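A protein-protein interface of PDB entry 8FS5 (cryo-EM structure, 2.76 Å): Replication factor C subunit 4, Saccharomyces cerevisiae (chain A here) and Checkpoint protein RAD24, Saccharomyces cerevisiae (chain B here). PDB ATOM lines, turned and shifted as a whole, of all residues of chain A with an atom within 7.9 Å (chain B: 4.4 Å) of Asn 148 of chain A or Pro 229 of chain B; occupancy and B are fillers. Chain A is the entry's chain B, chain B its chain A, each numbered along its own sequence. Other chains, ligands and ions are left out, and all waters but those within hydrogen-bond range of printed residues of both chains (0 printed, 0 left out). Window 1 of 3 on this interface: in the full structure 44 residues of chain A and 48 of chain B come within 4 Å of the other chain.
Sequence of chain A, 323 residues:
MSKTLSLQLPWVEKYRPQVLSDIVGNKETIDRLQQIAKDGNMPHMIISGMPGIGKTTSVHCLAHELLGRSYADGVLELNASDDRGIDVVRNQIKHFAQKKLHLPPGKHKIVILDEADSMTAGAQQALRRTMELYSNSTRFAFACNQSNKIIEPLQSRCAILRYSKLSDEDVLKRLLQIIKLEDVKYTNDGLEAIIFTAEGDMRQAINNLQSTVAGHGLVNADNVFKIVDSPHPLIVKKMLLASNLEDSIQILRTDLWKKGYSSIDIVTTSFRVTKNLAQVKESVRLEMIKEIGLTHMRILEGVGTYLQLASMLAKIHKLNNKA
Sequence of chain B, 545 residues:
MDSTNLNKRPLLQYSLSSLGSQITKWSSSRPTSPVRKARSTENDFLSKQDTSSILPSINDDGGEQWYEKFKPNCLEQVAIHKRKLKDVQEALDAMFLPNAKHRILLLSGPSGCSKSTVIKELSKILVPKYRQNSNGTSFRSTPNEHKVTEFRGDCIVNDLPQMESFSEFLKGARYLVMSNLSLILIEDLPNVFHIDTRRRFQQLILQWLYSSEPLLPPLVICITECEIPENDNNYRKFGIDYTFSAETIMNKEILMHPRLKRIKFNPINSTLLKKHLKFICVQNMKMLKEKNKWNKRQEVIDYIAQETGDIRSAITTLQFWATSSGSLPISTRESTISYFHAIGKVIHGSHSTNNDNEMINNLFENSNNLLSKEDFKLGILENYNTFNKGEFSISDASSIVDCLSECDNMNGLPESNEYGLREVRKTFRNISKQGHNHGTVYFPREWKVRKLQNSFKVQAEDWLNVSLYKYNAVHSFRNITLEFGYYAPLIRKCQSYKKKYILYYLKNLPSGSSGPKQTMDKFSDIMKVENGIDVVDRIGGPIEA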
ATOM      1  N   ILE A  46      21.007  21.510  15.981  1.00  0.00           N
ATOM      2  CA  ILE A  46      20.668  22.682  15.184  1.00  0.00           C
ATOM      3  C   ILE A  46      20.816  23.902  16.080  1.00  0.00           C
ATOM      4  O   ILE A  46      20.163  23.991  17.128  1.00  0.00           O
ATOM      5  CB  ILE A  46      19.247  22.595  14.605  1.00  0.00           C
ATOM      6  CG1 ILE A  46      19.118  21.384  13.679  1.00  0.00           C
ATOM      7  CG2 ILE A  46      18.895  23.877  13.866  1.00  0.00           C
ATOM      8  CD1 ILE A  46      17.750  21.238  13.051  1.00  0.00           C
ATOM      9  N   SER A  48      20.425  27.955  16.345  1.00  0.00           N
ATOM     10  CA  SER A  48      19.690  29.046  15.728  1.00  0.00           C
ATOM     11  C   SER A  48      19.756  30.283  16.613  1.00  0.00           C
ATOM     12  O   SER A  48      19.908  30.196  17.834  1.00  0.00           O
ATOM     13  CB  SER A  48      18.225  28.664  15.472  1.00  0.00           C
ATOM     14  OG  SER A  48      17.628  28.124  16.637  1.00  0.00           O
ATOM     15  N   ASP A 117      19.955  27.195   6.571  1.00  0.00           N
ATOM     16  CA  ASP A 117      18.668  27.769   6.200  1.00  0.00           C
ATOM     17  C   ASP A 117      18.585  28.137   4.724  1.00  0.00           C
ATOM     18  O   ASP A 117      17.478  28.351   4.220  1.00  0.00           O
ATOM     19  CB  ASP A 117      18.376  29.007   7.057  1.00  0.00           C
ATOM     20  CG  ASP A 117      19.609  29.850   7.309  1.00  0.00           C
ATOM     21  OD1 ASP A 117      20.732  29.331   7.151  1.00  0.00           O
ATOM     22  OD2 ASP A 117      19.453  31.037   7.665  1.00  0.00           O
ATOM     23  N   MET A 119      19.827  26.120   2.271  1.00  0.00           N
ATOM     24  CA  MET A 119      19.957  24.909   1.476  1.00  0.00           C
ATOM     25  C   MET A 119      18.642  24.576   0.783  1.00  0.00           C
ATOM     26  O   MET A 119      17.559  24.850   1.308  1.00  0.00           O
ATOM     27  CB  MET A 119      20.400  23.739   2.355  1.00  0.00           C
ATOM     28  CG  MET A 119      21.054  22.600   1.587  1.00  0.00           C
ATOM     29  SD  MET A 119      21.940  21.442   2.648  1.00  0.00           S
ATOM     30  CE  MET A 119      22.541  22.538   3.930  1.00  0.00           C
ATOM     31  N   THR A 120      18.744  23.985  -0.404  1.00  0.00           N
ATOM     32  CA  THR A 120      17.567  23.620  -1.175  1.00  0.00           C
ATOM     33  C   THR A 120      16.841  22.444  -0.522  1.00  0.00           C
ATOM     34  O   THR A 120      17.399  21.700   0.290  1.00  0.00           O
ATOM     35  CB  THR A 120      17.951  23.272  -2.613  1.00  0.00           C
ATOM     36  OG1 THR A 120      18.874  22.175  -2.611  1.00  0.00           O
ATOM     37  CG2 THR A 120      18.597  24.468  -3.296  1.00  0.00           C
ATOM     38  N   ALA A 121      15.568  22.286  -0.891  1.00  0.00           N
ATOM     39  CA  ALA A 121      14.729  21.241  -0.318  1.00  0.00           C
ATOM     40  C   ALA A 121      15.189  19.835  -0.683  1.00  0.00           C
ATOM     41  O   ALA A 121      15.127  18.941   0.167  1.00  0.00           O
ATOM     42  CB  ALA A 121      13.277  21.436  -0.754  1.00  0.00           C
ATOM     43  N   GLN A 124      18.172  18.898   1.430  1.00  0.00           N
ATOM     44  CA  GLN A 124      17.716  18.613   2.785  1.00  0.00           C
ATOM     45  C   GLN A 124      17.034  17.253   2.875  1.00  0.00           C
ATOM     46  O   GLN A 124      17.203  16.543   3.872  1.00  0.00           O
ATOM     47  CB  GLN A 124      16.773  19.718   3.262  1.00  0.00           C
ATOM     48  CG  GLN A 124      17.464  21.047   3.531  1.00  0.00           C
ATOM     49  CD  GLN A 124      16.647  21.962   4.421  1.00  0.00           C
ATOM     50  OE1 GLN A 124      15.957  21.506   5.332  1.00  0.00           O
ATOM     51  NE2 GLN A 124      16.719  23.261   4.159  1.00  0.00           N
ATOM     52  N   CYS A 144      22.099  27.975  11.787  1.00  0.00           N
ATOM     53  CA  CYS A 144      21.214  28.800  10.978  1.00  0.00           C
ATOM     54  C   CYS A 144      20.782  30.013  11.791  1.00  0.00           C
ATOM     55  O   CYS A 144      21.108  30.145  12.974  1.00  0.00           O
ATOM     56  CB  CYS A 144      19.997  27.997  10.506  1.00  0.00           C
ATOM     57  SG  CYS A 144      19.172  27.078  11.825  1.00  0.00           S
ATOM     58  N   ASN A 145      20.040  30.908  11.139  1.00  0.00           N
ATOM     59  CA  ASN A 145      19.470  32.079  11.790  1.00  0.00           C
ATOM     60  C   ASN A 145      17.977  31.962  12.043  1.00  0.00           C
ATOM     61  O   ASN A 145      17.472  32.585  12.979  1.00  0.00           O
ATOM     62  CB  ASN A 145      19.731  33.337  10.952  1.00  0.00           C
ATOM     63  CG  ASN A 145      21.106  33.929  11.195  1.00  0.00           C
ATOM     64  OD1 ASN A 145      21.277  35.148  11.185  1.00  0.00           O
ATOM     65  ND2 ASN A 145      22.095  33.069  11.413  1.00  0.00           N
ATOM     66  N   GLN A 146      17.262  31.185  11.234  1.00  0.00           N
ATOM     67  CA  GLN A 146      15.825  30.982  11.387  1.00  0.00           C
ATOM     68  C   GLN A 146      15.557  29.493  11.213  1.00  0.00           C
ATOM     69  O   GLN A 146      15.580  28.982  10.088  1.00  0.00           O
ATOM     70  CB  GLN A 146      15.044  31.827  10.377  1.00  0.00           C
ATOM     71  CG  GLN A 146      13.561  31.972  10.678  1.00  0.00           C
ATOM     72  CD  GLN A 146      12.682  31.576   9.508  1.00  0.00           C
ATOM     73  OE1 GLN A 146      12.998  31.864   8.354  1.00  0.00           O
ATOM     74  NE2 GLN A 146      11.565  30.926   9.804  1.00  0.00           N
ATOM     75  N   SER A 147      15.303  28.800  12.329  1.00  0.00           N
ATOM     76  CA  SER A 147      15.322  27.341  12.347  1.00  0.00           C
ATOM     77  C   SER A 147      14.190  26.709  11.547  1.00  0.00           C
ATOM     78  O   SER A 147      14.279  25.522  11.212  1.00  0.00           O
ATOM     79  CB  SER A 147      15.273  26.835  13.790  1.00  0.00           C
ATOM     80  OG  SER A 147      14.475  27.678  14.602  1.00  0.00           O
ATOM     81  N   ASN A 148      13.130  27.458  11.237  1.00  0.00           N
ATOM     82  CA  ASN A 148      12.022  26.880  10.483  1.00  0.00           C
ATOM     83  C   ASN A 148      12.408  26.594   9.036  1.00  0.00           C
ATOM     84  O   ASN A 148      11.716  25.832   8.351  1.00  0.00           O
ATOM     85  CB  ASN A 148      10.805  27.803  10.542  1.00  0.00           C
ATOM     86  CG  ASN A 148      10.740  28.600  11.829  1.00  0.00           C
ATOM     87  OD1 ASN A 148      10.744  29.831  11.813  1.00  0.00           O
ATOM     88  ND2 ASN A 148      10.679  27.900  12.956  1.00  0.00           N
ATOM     89  N   LYS A 149      13.502  27.187   8.553  1.00  0.00           N
ATOM     90  CA  LYS A 149      13.963  26.924   7.196  1.00  0.00           C
ATOM     91  C   LYS A 149      14.555  25.530   7.028  1.00  0.00           C
ATOM     92  O   LYS A 149      14.743  25.091   5.889  1.00  0.00           O
ATOM     93  CB  LYS A 149      14.990  27.972   6.774  1.00  0.00           C
ATOM     94  CG  LYS A 149      14.496  29.401   6.868  1.00  0.00           C
ATOM     95  CD  LYS A 149      13.552  29.730   5.725  1.00  0.00           C
ATOM     96  CE  LYS A 149      14.025  30.949   4.955  1.00  0.00           C
ATOM     97  NZ  LYS A 149      15.080  30.596   3.965  1.00  0.00           N
ATOM     98  N   ILE A 150      14.861  24.837   8.118  1.00  0.00           N
ATOM     99  CA  ILE A 150      15.276  23.441   8.062  1.00  0.00           C
ATOM    100  C   ILE A 150      14.032  22.577   8.214  1.00  0.00           C
ATOM    101  O   ILE A 150      13.234  22.783   9.137  1.00  0.00           O
ATOM    102  CB  ILE A 150      16.317  23.124   9.149  1.00  0.00           C
ATOM    103  CG1 ILE A 150      17.700  23.649   8.749  1.00  0.00           C
ATOM    104  CG2 ILE A 150      16.394  21.628   9.403  1.00  0.00           C
ATOM    105  CD1 ILE A 150      17.943  25.105   9.079  1.00  0.00           C
ATOM    106  N   ILE A 151      13.857  21.622   7.296  1.00  0.00           N
ATOM    107  CA  ILE A 151      12.630  20.838   7.264  1.00  0.00           C
ATOM    108  C   ILE A 151      12.479  20.022   8.548  1.00  0.00           C
ATOM    109  O   ILE A 151      13.460  19.599   9.171  1.00  0.00           O
ATOM    110  CB  ILE A 151      12.592  19.930   6.022  1.00  0.00           C
ATOM    111  CG1 ILE A 151      13.695  18.871   6.084  1.00  0.00           C
ATOM    112  CG2 ILE A 151      12.721  20.758   4.754  1.00  0.00           C
ATOM    113  CD1 ILE A 151      13.564  17.792   5.031  1.00  0.00           C
ATOM    114  N   GLU A 152      11.225  19.827   8.956  1.00  0.00           N
ATOM    115  CA  GLU A 152      10.851  19.121  10.178  1.00  0.00           C
ATOM    116  C   GLU A 152      11.401  17.695  10.254  1.00  0.00           C
ATOM    117  O   GLU A 152      11.801  17.271  11.346  1.00  0.00           O
ATOM    118  CB  GLU A 152       9.327  19.113  10.336  1.00  0.00           C
ATOM    119  CG  GLU A 152       8.714  20.498  10.463  1.00  0.00           C
ATOM    120  CD  GLU A 152       7.209  20.487  10.294  1.00  0.00           C
ATOM    121  OE1 GLU A 152       6.587  19.438  10.559  1.00  0.00           O
ATOM    122  OE2 GLU A 152       6.647  21.528   9.895  1.00  0.00           O
ATOM    123  N   GLN A 155      14.791  18.241  11.522  1.00  0.00           N
ATOM    124  CA  GLN A 155      14.795  18.690  12.909  1.00  0.00           C
ATOM    125  C   GLN A 155      14.435  17.575  13.881  1.00  0.00           C
ATOM    126  O   GLN A 155      14.827  17.640  15.051  1.00  0.00           O
ATOM    127  CB  GLN A 155      13.823  19.857  13.091  1.00  0.00           C
ATOM    128  CG  GLN A 155      14.061  21.019  12.145  1.00  0.00           C
ATOM    129  CD  GLN A 155      13.308  22.267  12.559  1.00  0.00           C
ATOM    130  OE1 GLN A 155      13.370  22.689  13.714  1.00  0.00           O
ATOM    131  NE2 GLN A 155      12.592  22.865  11.616  1.00  0.00           N
ATOM    132  N   ARG A 162      18.859  26.736  20.935  1.00  0.00           N
ATOM    133  CA  ARG A 162      18.512  28.100  20.560  1.00  0.00           C
ATOM    134  C   ARG A 162      19.386  29.075  21.337  1.00  0.00           C
ATOM    135  O   ARG A 162      19.388  29.065  22.573  1.00  0.00           O
ATOM    136  CB  ARG A 162      17.032  28.374  20.818  1.00  0.00           C
ATOM    137  CG  ARG A 162      16.100  27.428  20.080  1.00  0.00           C
ATOM    138  CD  ARG A 162      14.646  27.846  20.214  1.00  0.00           C
ATOM    139  NE  ARG A 162      13.744  26.709  20.089  1.00  0.00           N
ATOM    140  CZ  ARG A 162      13.281  26.242  18.936  1.00  0.00           C
ATOM    141  NH1 ARG A 162      13.616  26.795  17.782  1.00  0.00           N
ATOM    142  NH2 ARG A 162      12.463  25.193  18.943  1.00  0.00           N
ATOM    143  N   GLU B 227       6.029  21.007   5.492  1.00  0.00           N
ATOM    144  CA  GLU B 227       5.933  22.238   4.720  1.00  0.00           C
ATOM    145  C   GLU B 227       7.310  22.631   4.201  1.00  0.00           C
ATOM    146  O   GLU B 227       8.264  22.745   4.978  1.00  0.00           O
ATOM    147  CB  GLU B 227       5.342  23.355   5.576  1.00  0.00           C
ATOM    148  CG  GLU B 227       5.568  24.750   5.016  1.00  0.00           C
ATOM    149  CD  GLU B 227       4.295  25.573   4.969  1.00  0.00           C
ATOM    150  OE1 GLU B 227       4.050  26.233   3.938  1.00  0.00           O
ATOM    151  OE2 GLU B 227       3.542  25.561   5.965  1.00  0.00           O
ATOM    152  N   ILE B 228       7.415  22.835   2.892  1.00  0.00           N
ATOM    153  CA  ILE B 228       8.667  23.271   2.281  1.00  0.00           C
ATOM    154  C   ILE B 228       8.915  24.721   2.679  1.00  0.00           C
ATOM    155  O   ILE B 228       8.052  25.582   2.456  1.00  0.00           O
ATOM    156  CB  ILE B 228       8.638  23.103   0.754  1.00  0.00           C
ATOM    157  CG1 ILE B 228       8.520  21.622   0.387  1.00  0.00           C
ATOM    158  CG2 ILE B 228       9.883  23.710   0.127  1.00  0.00           C
ATOM    159  CD1 ILE B 228       9.550  20.742   1.066  1.00  0.00           C
ATOM    160  N   PRO B 229      10.066  25.032   3.274  1.00  0.00           N
ATOM    161  CA  PRO B 229      10.305  26.395   3.760  1.00  0.00           C
ATOM    162  C   PRO B 229      10.460  27.392   2.622  1.00  0.00           C
ATOM    163  O   PRO B 229      10.538  27.035   1.444  1.00  0.00           O
ATOM    164  CB  PRO B 229      11.606  26.259   4.560  1.00  0.00           C
ATOM    165  CG  PRO B 229      11.701  24.798   4.888  1.00  0.00           C
ATOM    166  CD  PRO B 229      11.133  24.109   3.688  1.00  0.00           C
ATOM    167  N   GLU B 230      10.504  28.668   2.998  1.00  0.00           N
ATOM    168  CA  GLU B 230      10.580  29.745   2.020  1.00  0.00           C
ATOM    169  C   GLU B 230      11.940  29.761   1.334  1.00  0.00           C
ATOM    170  O   GLU B 230      12.942  30.183   1.916  1.00  0.00           O
ATOM    171  CB  GLU B 230      10.310  31.094   2.692  1.00  0.00           C
ATOM    172  CG  GLU B 230       9.140  31.112   3.676  1.00  0.00           C
ATOM    173  CD  GLU B 230       9.527  30.678   5.080  1.00  0.00           C
ATOM    174  OE1 GLU B 230      10.178  29.622   5.228  1.00  0.00           O
ATOM    175  OE2 GLU B 230       9.176  31.397   6.039  1.00  0.00           O
ATOM    176  N   ASN B 231      11.960  29.300   0.085  1.00  0.00           N
ATOM    177  CA  ASN B 231      13.149  29.333  -0.755  1.00  0.00           C
ATOM    178  C   ASN B 231      12.713  29.429  -2.210  1.00  0.00           C
ATOM    179  O   ASN B 231      11.510  29.491  -2.484  1.00  0.00           O
ATOM    180  CB  ASN B 231      14.021  28.097  -0.524  1.00  0.00           C
ATOM    181  CG  ASN B 231      15.212  28.383   0.370  1.00  0.00           C
ATOM    182  OD1 ASN B 231      15.497  29.535   0.696  1.00  0.00           O
ATOM    183  ND2 ASN B 231      15.915  27.330   0.773  1.00  0.00           N
ATOM    184  N   LYS B 237       6.665  29.190  -7.813  1.00  0.00           N
ATOM    185  CA  LYS B 237       6.403  28.230  -6.749  1.00  0.00           C
ATOM    186  C   LYS B 237       5.181  27.382  -7.078  1.00  0.00           C
ATOM    187  O   LYS B 237       4.060  27.893  -7.148  1.00  0.00           O
ATOM    188  CB  LYS B 237       6.193  28.969  -5.428  1.00  0.00           C
ATOM    189  CG  LYS B 237       7.448  29.176  -4.599  1.00  0.00           C
ATOM    190  CD  LYS B 237       7.085  29.604  -3.185  1.00  0.00           C
ATOM    191  CE  LYS B 237       8.318  29.778  -2.318  1.00  0.00           C
ATOM    192  NZ  LYS B 237       9.117  28.524  -2.231  1.00  0.00           N
ATOM    193  N   GLU B 334      10.005  22.362  16.111  1.00  0.00           N
ATOM    194  CA  GLU B 334       8.867  23.224  15.830  1.00  0.00           C
ATOM    195  C   GLU B 334       7.986  22.597  14.760  1.00  0.00           C
ATOM    196  O   GLU B 334       8.482  22.097  13.745  1.00  0.00           O
ATOM    197  CB  GLU B 334       9.327  24.614  15.378  1.00  0.00           C
ATOM    198  CG  GLU B 334       9.608  25.612  16.503  1.00  0.00           C
ATOM    199  CD  GLU B 334       8.437  25.798  17.458  1.00  0.00           C
ATOM    200  OE1 GLU B 334       7.719  26.810  17.319  1.00  0.00           O
ATOM    201  OE2 GLU B 334       8.252  24.961  18.368  1.00  0.00           O
ATOM    202  N   GLU B 365       5.474  34.713  11.800  1.00  0.00           N
ATOM    203  CA  GLU B 365       6.892  34.372  11.855  1.00  0.00           C
ATOM    204  C   GLU B 365       7.131  32.925  11.442  1.00  0.00           C
ATOM    205  O   GLU B 365       8.038  32.636  10.653  1.00  0.00           O
ATOM    206  CB  GLU B 365       7.435  34.627  13.262  1.00  0.00           C
ATOM    207  CG  GLU B 365       8.941  34.472  13.386  1.00  0.00           C
ATOM    208  CD  GLU B 365       9.654  35.802  13.526  1.00  0.00           C
ATOM    209  OE1 GLU B 365       9.111  36.699  14.204  1.00  0.00           O
ATOM    210  OE2 GLU B 365      10.756  35.950  12.958  1.00  0.00           O
ATOM    211  N   ASN B 366       6.327  31.999  11.966  1.00  0.00           N
ATOM    212  CA  ASN B 366       6.560  30.580  11.732  1.00  0.00           C
ATOM    213  C   ASN B 366       5.876  30.055  10.477  1.00  0.00           C
ATOM    214  O   ASN B 366       6.309  29.033   9.931  1.00  0.00           O
ATOM    215  CB  ASN B 366       6.088  29.765  12.939  1.00  0.00           C
ATOM    216  CG  ASN B 366       6.570  30.341  14.256  1.00  0.00           C
ATOM    217  OD1 ASN B 366       7.435  31.216  14.284  1.00  0.00           O
ATOM    218  ND2 ASN B 366       6.010  29.852  15.356  1.00  0.00           N
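O of Glu 230 of chain B is in hydrogen-bond range of NZ of Lys 149 of chain A. The side-chain amide nitrogen (ND2) of Asn 231 of chain B lies within hydrogen-bond range of the backbone carbonyl oxygen (O) of Met 119 of chain A (3.0 Å). The side-chain amino group (NZ) of Lys 149 of chain A lies within hydrogen-bond range of the side-chain amide oxygen (OD1) of Asn 231 of chain B, at 3.5 Å.
Among the printed residues, merely in contact across the chains: Lys 149 of chain A with Pro 229 of chain B, Asn 148 of chain A with Pro 229 of chain B, Glu 152 of chain A with Glu 334 of chain B, Arg 162 of chain A with Glu 334 of chain B, Ile 151 of chain A with Pro 229 of chain B and Asp 117 of chain A with Asn 231 of chain B.
The backbone carbonyl oxygen (O) of Asp 117 of chain A is in hydrogen-bond range of the side-chain amino group (NZ) of Lys 149 of chain A, 3.3 Å away. O of Met 119 of chain A is in hydrogen-bond range of NE2 of Gln 124 of chain A, 3.4 Å away. The side-chain amide nitrogen (NE2) of Gln 124 of chain A sits at hydrogen-bond distance from the backbone carbonyl oxygen (O) of Lys 149 of chain A, 3.2 Å away. OE1 of Gln 124 of chain A lies within hydrogen-bond range of N of Ile 151 of chain A (2.9 Å). The side-chain amide nitrogen of Gln 146 of chain A sits at hydrogen-bond distance from the side-chain amide oxygen of Asn 148 of chain A (2.4 Å). The side-chain hydroxyl of Ser 147 of chain A is in hydrogen-bond range of the guanidinium group of Arg 162 of chain A, at 3.4 Å.
Of the printed residues of chain B, Asp 117 of chain A touches Asn 231 (3.9 Å). Of the printed residues of chain B, Met 119 of chain A touches Asn 231. Of chain B, only Pro 229 comes within 4 Å of Asn 148 of chain A. Printed residues of chain B within 4 Å of Glu 152 of chain A: Glu 334. Of the printed residues of chain B, Arg 162 of chain A touches Glu 334 (3.8 Å). Glu 227 of chain B touches none of the printed residues of chain A. Pro 229 of chain B touches three residues of chain A. Printed residues of chain A within 4 Å of Asn 231 of chain B: Asp 117 (3.9 Å), Met 119 (3.0 Å) and Lys 149 (3.5 Å). Glu 365 of chain B touches none of the printed residues of chain A. The nearest residue of chain A that does not touch Pro 229 of chain B is Ile 150 of chain A (4.5 Å).
Hydrophobic or aromatic side chains of chain B within 4 Å of the printed part of chain A: Pro 229. Along chain B the printed residues that touch a printed residue of chain A span positions 229 to 334. Printed residues of chain A that touch a printed residue of chain B: Asp 117, Met 119, Asn 148, Lys 149, Ile 151, Glu 152 and Arg 162. Among the printed residues, 9 pairs touch across the chains. Among the printed residues, no Asp or Glu carboxylate lies within 4 Å of a Lys or Arg side-chain nitrogen of the other chain.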
